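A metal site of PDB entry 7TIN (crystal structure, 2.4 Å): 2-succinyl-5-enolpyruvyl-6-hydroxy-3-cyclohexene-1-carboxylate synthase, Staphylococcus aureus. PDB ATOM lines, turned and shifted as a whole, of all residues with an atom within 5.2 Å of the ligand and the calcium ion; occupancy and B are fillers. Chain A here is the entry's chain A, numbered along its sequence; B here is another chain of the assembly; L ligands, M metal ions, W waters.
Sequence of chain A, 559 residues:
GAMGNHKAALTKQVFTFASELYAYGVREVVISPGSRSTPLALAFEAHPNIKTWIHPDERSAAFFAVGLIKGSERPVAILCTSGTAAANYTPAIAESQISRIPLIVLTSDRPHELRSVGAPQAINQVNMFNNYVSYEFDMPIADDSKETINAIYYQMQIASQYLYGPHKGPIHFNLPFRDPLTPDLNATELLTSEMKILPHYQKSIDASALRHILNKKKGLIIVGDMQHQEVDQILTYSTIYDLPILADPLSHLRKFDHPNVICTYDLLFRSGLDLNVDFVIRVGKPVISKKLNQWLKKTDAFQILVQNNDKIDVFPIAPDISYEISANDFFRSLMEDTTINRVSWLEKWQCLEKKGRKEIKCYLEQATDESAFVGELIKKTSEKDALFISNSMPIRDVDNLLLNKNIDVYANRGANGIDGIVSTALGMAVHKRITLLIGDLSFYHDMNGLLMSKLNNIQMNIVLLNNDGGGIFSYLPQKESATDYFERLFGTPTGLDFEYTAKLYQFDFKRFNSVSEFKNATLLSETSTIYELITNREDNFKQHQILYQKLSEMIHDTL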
ATOM      1  N   GLU A 370     -24.366 -21.552 -25.550  1.00  0.00           N
ATOM      2  CA  GLU A 370     -24.440 -20.248 -24.895  1.00  0.00           C
ATOM      3  C   GLU A 370     -24.242 -19.106 -25.887  1.00  0.00           C
ATOM      4  O   GLU A 370     -24.859 -18.039 -25.741  1.00  0.00           O
ATOM      5  CB  GLU A 370     -23.403 -20.164 -23.774  1.00  0.00           C
ATOM      6  CG  GLU A 370     -23.615 -19.015 -22.809  1.00  0.00           C
ATOM      7  CD  GLU A 370     -22.679 -19.051 -21.610  1.00  0.00           C
ATOM      8  OE1 GLU A 370     -21.555 -18.518 -21.696  1.00  0.00           O
ATOM      9  OE2 GLU A 370     -23.069 -19.643 -20.570  1.00  0.00           O
ATOM     10  N   SER A 390     -20.832  -8.552 -18.737  1.00  0.00           N
ATOM     11  CA  SER A 390     -19.953  -9.022 -17.683  1.00  0.00           C
ATOM     12  C   SER A 390     -18.589  -9.376 -18.268  1.00  0.00           C
ATOM     13  O   SER A 390     -18.350  -9.278 -19.471  1.00  0.00           O
ATOM     14  CB  SER A 390     -20.591 -10.221 -16.973  1.00  0.00           C
ATOM     15  OG  SER A 390     -19.862 -10.583 -15.821  1.00  0.00           O
ATOM     16  N   ASN A 391     -17.680  -9.801 -17.399  1.00  0.00           N
ATOM     17  CA  ASN A 391     -16.392 -10.315 -17.863  1.00  0.00           C
ATOM     18  C   ASN A 391     -16.523 -11.828 -18.070  1.00  0.00           C
ATOM     19  O   ASN A 391     -17.644 -12.346 -18.164  1.00  0.00           O
ATOM     20  CB  ASN A 391     -15.284  -9.918 -16.881  1.00  0.00           C
ATOM     21  CG  ASN A 391     -15.037  -8.415 -16.878  1.00  0.00           C
ATOM     22  OD1 ASN A 391     -15.120  -7.756 -17.918  1.00  0.00           O
ATOM     23  ND2 ASN A 391     -14.742  -7.877 -15.704  1.00  0.00           N
ATOM     24  N   SER A 392     -15.404 -12.532 -18.154  1.00  0.00           N
ATOM     25  CA  SER A 392     -15.381 -13.973 -18.449  1.00  0.00           C
ATOM     26  C   SER A 392     -15.946 -14.170 -19.860  1.00  0.00           C
ATOM     27  O   SER A 392     -15.716 -13.321 -20.741  1.00  0.00           O
ATOM     28  CB  SER A 392     -16.098 -14.745 -17.356  1.00  0.00           C
ATOM     29  OG  SER A 392     -15.618 -16.078 -17.277  1.00  0.00           O
ATOM     30  N   MET A 393     -16.681 -15.256 -20.127  1.00  0.00           N
ATOM     31  CA  MET A 393     -17.095 -15.577 -21.485  1.00  0.00           C
ATOM     32  C   MET A 393     -17.978 -14.529 -22.161  1.00  0.00           C
ATOM     33  O   MET A 393     -17.782 -14.300 -23.372  1.00  0.00           O
ATOM     34  CB  MET A 393     -17.796 -16.938 -21.512  1.00  0.00           C
ATOM     35  CG  MET A 393     -16.848 -18.131 -21.512  1.00  0.00           C
ATOM     36  SD  MET A 393     -15.250 -17.789 -22.292  1.00  0.00           S
ATOM     37  CE  MET A 393     -15.624 -17.987 -24.025  1.00  0.00           C
ATOM     38  N   PRO A 394     -18.952 -13.889 -21.498  1.00  0.00           N
ATOM     39  CA  PRO A 394     -19.853 -12.969 -22.226  1.00  0.00           C
ATOM     40  C   PRO A 394     -19.133 -11.884 -23.009  1.00  0.00           C
ATOM     41  O   PRO A 394     -19.528 -11.595 -24.146  1.00  0.00           O
ATOM     42  CB  PRO A 394     -20.720 -12.389 -21.118  1.00  0.00           C
ATOM     43  CG  PRO A 394     -20.814 -13.481 -20.127  1.00  0.00           C
ATOM     44  CD  PRO A 394     -19.448 -14.121 -20.119  1.00  0.00           C
ATOM     45  N   ASN A 416     -10.747  -6.359 -14.919  1.00  0.00           N
ATOM     46  CA  ASN A 416     -11.427  -7.558 -15.406  1.00  0.00           C
ATOM     47  C   ASN A 416     -11.933  -8.417 -14.260  1.00  0.00           C
ATOM     48  O   ASN A 416     -11.773  -9.647 -14.246  1.00  0.00           O
ATOM     49  CB  ASN A 416     -10.514  -8.360 -16.334  1.00  0.00           C
ATOM     50  CG  ASN A 416     -10.020  -7.535 -17.516  1.00  0.00           C
ATOM     51  OD1 ASN A 416     -10.655  -6.562 -17.919  1.00  0.00           O
ATOM     52  ND2 ASN A 416      -8.888  -7.938 -18.077  1.00  0.00           N
ATOM     53  N   GLY A 417     -12.539  -7.775 -13.265  1.00  0.00           N
ATOM     54  CA  GLY A 417     -13.053  -8.481 -12.123  1.00  0.00           C
ATOM     55  C   GLY A 417     -14.464  -9.020 -12.369  1.00  0.00           C
ATOM     56  O   GLY A 417     -15.218  -8.489 -13.170  1.00  0.00           O
ATOM     57  N   ILE A 418     -14.788 -10.099 -11.646  1.00  0.00           N
ATOM     58  CA  ILE A 418     -16.153 -10.603 -11.635  1.00  0.00           C
ATOM     59  C   ILE A 418     -16.956 -10.029 -10.481  1.00  0.00           C
ATOM     60  O   ILE A 418     -18.125 -10.396 -10.291  1.00  0.00           O
ATOM     61  CB  ILE A 418     -16.173 -12.146 -11.564  1.00  0.00           C
ATOM     62  CG1 ILE A 418     -15.626 -12.614 -10.212  1.00  0.00           C
ATOM     63  CG2 ILE A 418     -15.393 -12.738 -12.728  1.00  0.00           C
ATOM     64  CD1 ILE A 418     -15.479 -14.120 -10.102  1.00  0.00           C
ATOM     65  N   ASP A 419     -16.370  -9.125  -9.695  1.00  0.00           N
ATOM     66  CA  ASP A 419     -17.060  -8.490  -8.584  1.00  0.00           C
ATOM     67  C   ASP A 419     -17.698  -7.184  -9.038  1.00  0.00           C
ATOM     68  O   ASP A 419     -17.221  -6.513  -9.947  1.00  0.00           O
ATOM     69  CB  ASP A 419     -16.094  -8.222  -7.422  1.00  0.00           C
ATOM     70  CG  ASP A 419     -14.726  -7.726  -7.883  1.00  0.00           C
ATOM     71  OD1 ASP A 419     -14.488  -7.607  -9.109  1.00  0.00           O
ATOM     72  OD2 ASP A 419     -13.875  -7.449  -7.006  1.00  0.00           O
ATOM     73  N   GLY A 439     -22.696 -13.871 -16.210  1.00  0.00           N
ATOM     74  CA  GLY A 439     -22.623 -15.266 -15.833  1.00  0.00           C
ATOM     75  C   GLY A 439     -23.008 -15.497 -14.372  1.00  0.00           C
ATOM     76  O   GLY A 439     -23.123 -14.563 -13.577  1.00  0.00           O
ATOM     77  N   ASP A 440     -23.215 -16.773 -14.033  1.00  0.00           N
ATOM     78  CA  ASP A 440     -23.810 -17.094 -12.728  1.00  0.00           C
ATOM     79  C   ASP A 440     -22.846 -16.798 -11.583  1.00  0.00           C
ATOM     80  O   ASP A 440     -23.274 -16.337 -10.520  1.00  0.00           O
ATOM     81  CB  ASP A 440     -24.262 -18.551 -12.696  1.00  0.00           C
ATOM     82  CG  ASP A 440     -23.203 -19.510 -13.224  1.00  0.00           C
ATOM     83  OD1 ASP A 440     -22.980 -19.511 -14.452  1.00  0.00           O
ATOM     84  OD2 ASP A 440     -22.612 -20.258 -12.413  1.00  0.00           O
ATOM     85  N   LEU A 441     -21.554 -17.058 -11.762  1.00  0.00           N
ATOM     86  CA  LEU A 441     -20.612 -16.817 -10.674  1.00  0.00           C
ATOM     87  C   LEU A 441     -20.492 -15.327 -10.367  1.00  0.00           C
ATOM     88  O   LEU A 441     -20.475 -14.931  -9.200  1.00  0.00           O
ATOM     89  CB  LEU A 441     -19.247 -17.430 -10.990  1.00  0.00           C
ATOM     90  CG  LEU A 441     -19.164 -18.959 -10.897  1.00  0.00           C
ATOM     91  CD1 LEU A 441     -17.744 -19.451 -11.140  1.00  0.00           C
ATOM     92  CD2 LEU A 441     -19.682 -19.469  -9.553  1.00  0.00           C
ATOM     93  N   SER A 442     -20.432 -14.475 -11.404  1.00  0.00           N
ATOM     94  CA  SER A 442     -20.439 -13.039 -11.150  1.00  0.00           C
ATOM     95  C   SER A 442     -21.784 -12.582 -10.605  1.00  0.00           C
ATOM     96  O   SER A 442     -21.838 -11.674  -9.770  1.00  0.00           O
ATOM     97  CB  SER A 442     -20.072 -12.246 -12.407  1.00  0.00           C
ATOM     98  OG  SER A 442     -19.646 -13.090 -13.453  1.00  0.00           O
ATOM     99  N   HIS A 445     -21.541 -13.241  -7.128  1.00  0.00           N
ATOM    100  CA  HIS A 445     -20.561 -12.384  -6.463  1.00  0.00           C
ATOM    101  C   HIS A 445     -21.203 -11.091  -5.955  1.00  0.00           C
ATOM    102  O   HIS A 445     -21.019 -10.703  -4.803  1.00  0.00           O
ATOM    103  CB  HIS A 445     -19.399 -12.082  -7.410  1.00  0.00           C
ATOM    104  CG  HIS A 445     -18.062 -12.071  -6.732  1.00  0.00           C
ATOM    105  ND1 HIS A 445     -17.589 -10.979  -6.026  1.00  0.00           N
ATOM    106  CD2 HIS A 445     -17.092 -13.006  -6.659  1.00  0.00           C
ATOM    107  CE1 HIS A 445     -16.390 -11.248  -5.552  1.00  0.00           C
ATOM    108  NE2 HIS A 445     -16.060 -12.477  -5.920  1.00  0.00           N
ATOM    109  N   LEU A 465     -26.829 -15.919 -17.743  1.00  0.00           N
ATOM    110  CA  LEU A 465     -26.282 -17.116 -18.365  1.00  0.00           C
ATOM    111  C   LEU A 465     -25.777 -18.032 -17.262  1.00  0.00           C
ATOM    112  O   LEU A 465     -24.726 -17.765 -16.654  1.00  0.00           O
ATOM    113  CB  LEU A 465     -25.167 -16.769 -19.345  1.00  0.00           C
ATOM    114  CG  LEU A 465     -25.572 -15.973 -20.574  1.00  0.00           C
ATOM    115  CD1 LEU A 465     -24.368 -15.715 -21.462  1.00  0.00           C
ATOM    116  CD2 LEU A 465     -26.671 -16.691 -21.340  1.00  0.00           C
ATOM    117  N   ASN A 467     -24.435 -21.631 -16.450  1.00  0.00           N
ATOM    118  CA  ASN A 467     -23.906 -22.944 -16.752  1.00  0.00           C
ATOM    119  C   ASN A 467     -23.320 -23.612 -15.509  1.00  0.00           C
ATOM    120  O   ASN A 467     -22.550 -24.574 -15.631  1.00  0.00           O
ATOM    121  CB  ASN A 467     -22.878 -22.872 -17.871  1.00  0.00           C
ATOM    122  CG  ASN A 467     -21.825 -21.799 -17.653  1.00  0.00           C
ATOM    123  OD1 ASN A 467     -21.242 -21.690 -16.577  1.00  0.00           O
ATOM    124  ND2 ASN A 467     -21.589 -20.993 -18.681  1.00  0.00           N
ATOM    125  N   ASP A 468     -23.655 -23.103 -14.326  1.00  0.00           N
ATOM    126  CA  ASP A 468     -23.267 -23.690 -13.042  1.00  0.00           C
ATOM    127  C   ASP A 468     -21.753 -23.910 -12.951  1.00  0.00           C
ATOM    128  O   ASP A 468     -21.257 -25.038 -12.891  1.00  0.00           O
ATOM    129  CB  ASP A 468     -24.032 -24.993 -12.804  1.00  0.00           C
ATOM    130  CG  ASP A 468     -24.190 -25.316 -11.329  1.00  0.00           C
ATOM    131  OD1 ASP A 468     -24.195 -24.377 -10.503  1.00  0.00           O
ATOM    132  OD2 ASP A 468     -24.299 -26.520 -10.987  1.00  0.00           O
ATOM    133  N   GLY A 469     -21.032 -22.808 -12.939  1.00  0.00           N
ATOM    134  CA  GLY A 469     -19.611 -22.837 -12.740  1.00  0.00           C
ATOM    135  C   GLY A 469     -18.900 -21.826 -13.620  1.00  0.00           C
ATOM    136  O   GLY A 469     -19.524 -20.940 -14.194  1.00  0.00           O
ATOM    137  N   GLY A 470     -17.580 -21.981 -13.708  1.00  0.00           N
ATOM    138  CA  GLY A 470     -16.764 -21.084 -14.499  1.00  0.00           C
ATOM    139  C   GLY A 470     -16.409 -21.646 -15.862  1.00  0.00           C
ATOM    140  O   GLY A 470     -15.436 -22.400 -16.001  1.00  0.00           O
ATOM    141  N   GLY A 471     -17.202 -21.281 -16.881  1.00  0.00           N
ATOM    142  CA  GLY A 471     -17.018 -21.870 -18.190  1.00  0.00           C
ATOM    143  C   GLY A 471     -15.719 -21.488 -18.877  1.00  0.00           C
ATOM    144  O   GLY A 471     -15.186 -22.260 -19.666  1.00  0.00           O
ATOM    145  N   ILE A 472     -15.192 -20.291 -18.586  1.00  0.00           N
ATOM    146  CA  ILE A 472     -13.990 -19.822 -19.258  1.00  0.00           C
ATOM    147  C   ILE A 472     -12.819 -20.759 -19.031  1.00  0.00           C
ATOM    148  O   ILE A 472     -11.906 -20.848 -19.863  1.00  0.00           O
ATOM    149  CB  ILE A 472     -13.654 -18.375 -18.814  1.00  0.00           C
ATOM    150  CG1 ILE A 472     -12.648 -17.743 -19.772  1.00  0.00           C
ATOM    151  CG2 ILE A 472     -13.109 -18.348 -17.380  1.00  0.00           C
ATOM    152  CD1 ILE A 472     -12.756 -16.230 -19.861  1.00  0.00           C
ATOM    153  N   PHE A 473     -12.818 -21.499 -17.913  1.00  0.00           N
ATOM    154  CA  PHE A 473     -11.687 -22.375 -17.617  1.00  0.00           C
ATOM    155  C   PHE A 473     -11.714 -23.655 -18.440  1.00  0.00           C
ATOM    156  O   PHE A 473     -10.727 -24.399 -18.413  1.00  0.00           O
ATOM    157  CB  PHE A 473     -11.651 -22.697 -16.126  1.00  0.00           C
ATOM    158  CG  PHE A 473     -11.541 -21.477 -15.257  1.00  0.00           C
ATOM    159  CD1 PHE A 473     -10.530 -20.553 -15.466  1.00  0.00           C
ATOM    160  CD2 PHE A 473     -12.463 -21.236 -14.250  1.00  0.00           C
ATOM    161  CE1 PHE A 473     -10.435 -19.419 -14.680  1.00  0.00           C
ATOM    162  CE2 PHE A 473     -12.360 -20.110 -13.455  1.00  0.00           C
ATOM    163  CZ  PHE A 473     -11.349 -19.194 -13.671  1.00  0.00           C
ATOM    164  N   PRO B  33     -11.177 -19.526  -6.991  1.00  0.00           N
ATOM    165  CA  PRO B  33     -10.854 -19.916  -8.378  1.00  0.00           C
ATOM    166  C   PRO B  33     -10.162 -18.796  -9.139  1.00  0.00           C
ATOM    167  O   PRO B  33     -10.477 -17.613  -8.974  1.00  0.00           O
ATOM    168  CB  PRO B  33     -12.228 -20.228  -8.977  1.00  0.00           C
ATOM    169  CG  PRO B  33     -13.199 -19.474  -8.127  1.00  0.00           C
ATOM    170  CD  PRO B  33     -12.625 -19.505  -6.749  1.00  0.00           C
ATOM    171  N   GLY B  34      -9.209 -19.191  -9.980  1.00  0.00           N
ATOM    172  CA  GLY B  34      -8.516 -18.262 -10.857  1.00  0.00           C
ATOM    173  C   GLY B  34      -7.501 -19.032 -11.678  1.00  0.00           C
ATOM    174  O   GLY B  34      -7.144 -20.172 -11.373  1.00  0.00           O
ATOM    175  N   GLU B  58     -14.107 -13.943  -2.599  1.00  0.00           N
ATOM    176  CA  GLU B  58     -12.888 -13.772  -1.821  1.00  0.00           C
ATOM    177  C   GLU B  58     -13.155 -13.035  -0.506  1.00  0.00           C
ATOM    178  O   GLU B  58     -12.555 -13.365   0.530  1.00  0.00           O
ATOM    179  CB  GLU B  58     -11.832 -13.038  -2.642  1.00  0.00           C
ATOM    180  CG  GLU B  58     -11.252 -13.831  -3.795  1.00  0.00           C
ATOM    181  CD  GLU B  58     -12.088 -13.732  -5.069  1.00  0.00           C
ATOM    182  OE1 GLU B  58     -13.145 -13.073  -5.044  1.00  0.00           O
ATOM    183  OE2 GLU B  58     -11.682 -14.317  -6.099  1.00  0.00           O
ATOM    184  N   THR B  81      -6.273 -15.541  -7.102  1.00  0.00           N
ATOM    185  CA  THR B  81      -5.624 -15.158  -8.344  1.00  0.00           C
ATOM    186  C   THR B  81      -5.325 -13.659  -8.339  1.00  0.00           C
ATOM    187  O   THR B  81      -5.692 -12.927  -7.413  1.00  0.00           O
ATOM    188  CB  THR B  81      -6.510 -15.559  -9.528  1.00  0.00           C
ATOM    189  OG1 THR B  81      -5.745 -15.534 -10.742  1.00  0.00           O
ATOM    190  CG2 THR B  81      -7.714 -14.633  -9.637  1.00  0.00           C
ATOM    191  N   THR B  84      -8.331  -7.795  -8.606  1.00  0.00           N
ATOM    192  CA  THR B  84      -9.240  -7.395  -7.535  1.00  0.00           C
ATOM    193  C   THR B  84      -9.624  -8.549  -6.622  1.00  0.00           C
ATOM    194  O   THR B  84     -10.219  -8.291  -5.565  1.00  0.00           O
ATOM    195  CB  THR B  84     -10.523  -6.770  -8.097  1.00  0.00           C
ATOM    196  OG1 THR B  84     -11.081  -7.629  -9.111  1.00  0.00           O
ATOM    197  CG2 THR B  84     -10.231  -5.397  -8.694  1.00  0.00           C
ATOM    198  N   ALA B  85      -9.333  -9.784  -7.011  1.00  0.00           N
ATOM    199  CA  ALA B  85      -9.513 -10.903  -6.089  1.00  0.00           C
ATOM    200  C   ALA B  85      -8.775 -10.661  -4.783  1.00  0.00           C
ATOM    201  O   ALA B  85      -9.332 -10.881  -3.694  1.00  0.00           O
ATOM    202  CB  ALA B  85      -9.025 -12.204  -6.743  1.00  0.00           C
ATOM    203  N   ASN B  88     -10.356  -7.873  -2.457  1.00  0.00           N
ATOM    204  CA  ASN B  88     -11.458  -8.321  -1.620  1.00  0.00           C
ATOM    205  C   ASN B  88     -11.006  -8.914  -0.288  1.00  0.00           C
ATOM    206  O   ASN B  88     -11.840  -9.087   0.602  1.00  0.00           O
ATOM    207  CB  ASN B  88     -12.306  -9.355  -2.367  1.00  0.00           C
ATOM    208  CG  ASN B  88     -13.200  -8.722  -3.434  1.00  0.00           C
ATOM    209  OD1 ASN B  88     -14.324  -8.314  -3.145  1.00  0.00           O
ATOM    210  ND2 ASN B  88     -12.705  -8.659  -4.658  1.00  0.00           N
ATOM    211  N   GLN B 121      -5.877  -6.211 -15.669  1.00  0.00           N
ATOM    212  CA  GLN B 121      -5.917  -7.018 -14.459  1.00  0.00           C
ATOM    213  C   GLN B 121      -4.621  -6.908 -13.664  1.00  0.00           C
ATOM    214  O   GLN B 121      -4.250  -7.819 -12.913  1.00  0.00           O
ATOM    215  CB  GLN B 121      -6.218  -8.490 -14.774  1.00  0.00           C
ATOM    216  CG  GLN B 121      -6.833  -9.283 -13.635  1.00  0.00           C
ATOM    217  CD  GLN B 121      -7.316 -10.640 -14.081  1.00  0.00           C
ATOM    218  OE1 GLN B 121      -8.135 -10.750 -14.993  1.00  0.00           O
ATOM    219  NE2 GLN B 121      -6.810 -11.686 -13.443  1.00  0.00           N
HETATM  220  N1  LIG L   1     -12.019 -13.215  -8.601  1.00  0.00           N
HETATM  221  C1  LIG L   1     -12.347 -12.016  -9.121  1.00  0.00           C
HETATM  222  C2  LIG L   1     -12.817 -10.963  -8.168  1.00  0.00           C
HETATM  223  N2  LIG L   1     -12.303 -11.690 -10.412  1.00  0.00           N
HETATM  224  C3  LIG L   1     -11.886 -12.627 -11.281  1.00  0.00           C
HETATM  225  N3  LIG L   1     -11.845 -12.272 -12.575  1.00  0.00           N
HETATM  226  C4  LIG L   1     -11.515 -13.926 -10.834  1.00  0.00           C
HETATM  227  C5  LIG L   1     -11.607 -14.138  -9.486  1.00  0.00           C
HETATM  228  C6  LIG L   1     -11.047 -15.021 -11.770  1.00  0.00           C
HETATM  229  N4  LIG L   1     -12.059 -15.390 -12.789  1.00  0.00           N
HETATM  230  C7  LIG L   1     -12.047 -14.932 -14.030  1.00  0.00           C
HETATM  231  S1  LIG L   1     -13.341 -15.503 -14.930  1.00  0.00           S
HETATM  232  C8  LIG L   1     -13.924 -16.411 -13.577  1.00  0.00           C
HETATM  233  C9  LIG L   1     -13.129 -16.232 -12.501  1.00  0.00           C
HETATM  234  C10 LIG L   1     -13.284 -16.829 -11.144  1.00  0.00           C
HETATM  235  C11 LIG L   1     -15.171 -17.243 -13.691  1.00  0.00           C
HETATM  236  C12 LIG L   1     -16.436 -16.402 -13.733  1.00  0.00           C
HETATM  237  O1  LIG L   1     -17.544 -17.264 -14.089  1.00  0.00           O
HETATM  238  P1  LIG L   1     -18.927 -16.747 -14.630  1.00  0.00           P
HETATM  239  O2  LIG L   1     -20.012 -17.718 -14.171  1.00  0.00           O
HETATM  240  O3  LIG L   1     -19.164 -15.329 -14.267  1.00  0.00           O
HETATM  241  O4  LIG L   1     -18.779 -16.923 -16.180  1.00  0.00           O
HETATM  242  P2  LIG L   1     -18.288 -18.005 -17.236  1.00  0.00           P
HETATM  243  O5  LIG L   1     -19.156 -19.233 -16.969  1.00  0.00           O
HETATM  244  O6  LIG L   1     -18.674 -17.406 -18.578  1.00  0.00           O
HETATM  245  O7  LIG L   1     -16.827 -18.285 -17.092  1.00  0.00           O
HETATM  246 CA    CA M   1     -20.882 -19.605 -15.482  1.00  0.00          CA
HETATM  247  O   HOH W   1     -21.966 -18.312 -17.154  1.00  0.00           O
HETATM  248  O   HOH W   2     -13.534 -15.982  -7.638  1.00  0.00           O
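The backbone NH (N) of Asp 440 lies close to an oxygen (O2) of the ligand (3.3 Å). An oxygen (O3) of the ligand lies within hydrogen-bond range of the backbone NH (N) of Ser 442 (3.2 Å). OG of Ser 442 lies within hydrogen-bond range of O3 of the ligand (2.4 Å). OG of Ser 392 lies within hydrogen-bond range of O7 of the ligand (2.5 Å). The side-chain carboxylate (OE2) of Glu 58 of chain B sits at hydrogen-bond distance from a nitrogen (N1) of the ligand (2.8 Å). N of Gly 471 is in hydrogen-bond range of O7 of the ligand (3.0 Å). N of Leu 441 sits close to O2 of the ligand (2.9 Å). N of Ile 472 is in hydrogen-bond range of O7 of the ligand (3.0 Å). The backbone NH (N) of Met 393 lies close to an oxygen (O6) of the ligand, at 3.3 Å. A nitrogen (N3) of the ligand is in hydrogen-bond range of the backbone carbonyl oxygen of Asn 416 (3.1 Å). N2 of the ligand lies within hydrogen-bond range of N of Ile 418, at 3.2 Å.
The calcium ion is bound by the backbone carbonyl oxygen of Gly 469 (2.3 Å), an oxygen (O5) of the ligand (2.3 Å), the side-chain carboxylate of Asp 440 (2.3 Å), water W1 (2.4 Å), the side-chain amide oxygen of Asn 467 (2.4 Å) and an oxygen (O2) of the ligand (2.5 Å). The calcium ion has six donor atoms within binding distance.
Residues that only touch the ligand: Pro 394 (3.7 Å), Gly 417 (3.7 Å), Asp 419 (3.8 Å), Gly 439 (3.7 Å), Gly 470 (3.6 Å), Phe 473 (3.6 Å), Pro 33 of chain B (3.6 Å), Thr 81 of chain B (3.9 Å), Thr 84 of chain B (3.9 Å) and Ala 85 of chain B (3.7 Å). Hydrophobic or aromatic side chains within 4 Å of the ligand: Met 393, Pro 394, Ile 418, Leu 441, Ile 472, Phe 473 and Ala 85 of chain B. The nearest printed residue that does not touch the ligand is Asn 88 of chain B (4.2 Å).
N of Asp 440 sits at hydrogen-bond distance from O of Leu 465, at 3.2 Å. The side-chain carboxylate (OE2) of Glu 370 is in hydrogen-bond range of the side-chain amide nitrogen (ND2) of Asn 467, 2.8 Å away. The side-chain hydroxyl (OG) of Ser 442 lies within hydrogen-bond range of the side-chain hydroxyl (OG) of Ser 390. OE1 of Glu 58 of chain B lies within hydrogen-bond range of NE2 of His 445 (3.1 Å). The backbone carbonyl oxygen (O) of Gly 417 sits at hydrogen-bond distance from the side-chain amide nitrogen (ND2) of Asn 391, at 2.6 Å. The side-chain carboxylate of Asp 419 sits at hydrogen-bond distance from the side-chain hydroxyl of Thr 84 of chain B, 3.4 Å away. ND2 of Asn 88 of chain B lies within hydrogen-bond range of OD2 of Asp 419, 2.9 Å away. The side-chain amide nitrogen (ND2) of Asn 88 of chain B lies within hydrogen-bond range of the backbone carbonyl oxygen (O) of Thr 84 of chain B (2.7 Å).
Within 4 Å of the calcium ion: Asp 440, Asn 467 and Gly 469. The nearest printed residue that does not touch the calcium ion is Gly 471 (4.3 Å).
Water W1 bridges the backbone carbonyl oxygen of Leu 465 and the side-chain amide nitrogen of Asn 467. Water W2 lies within hydrogen-bond range of the side-chain carboxylate (OE2) of Glu 58 of chain B (2.9 Å) and a nitrogen (N1) of the ligand (3.3 Å).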
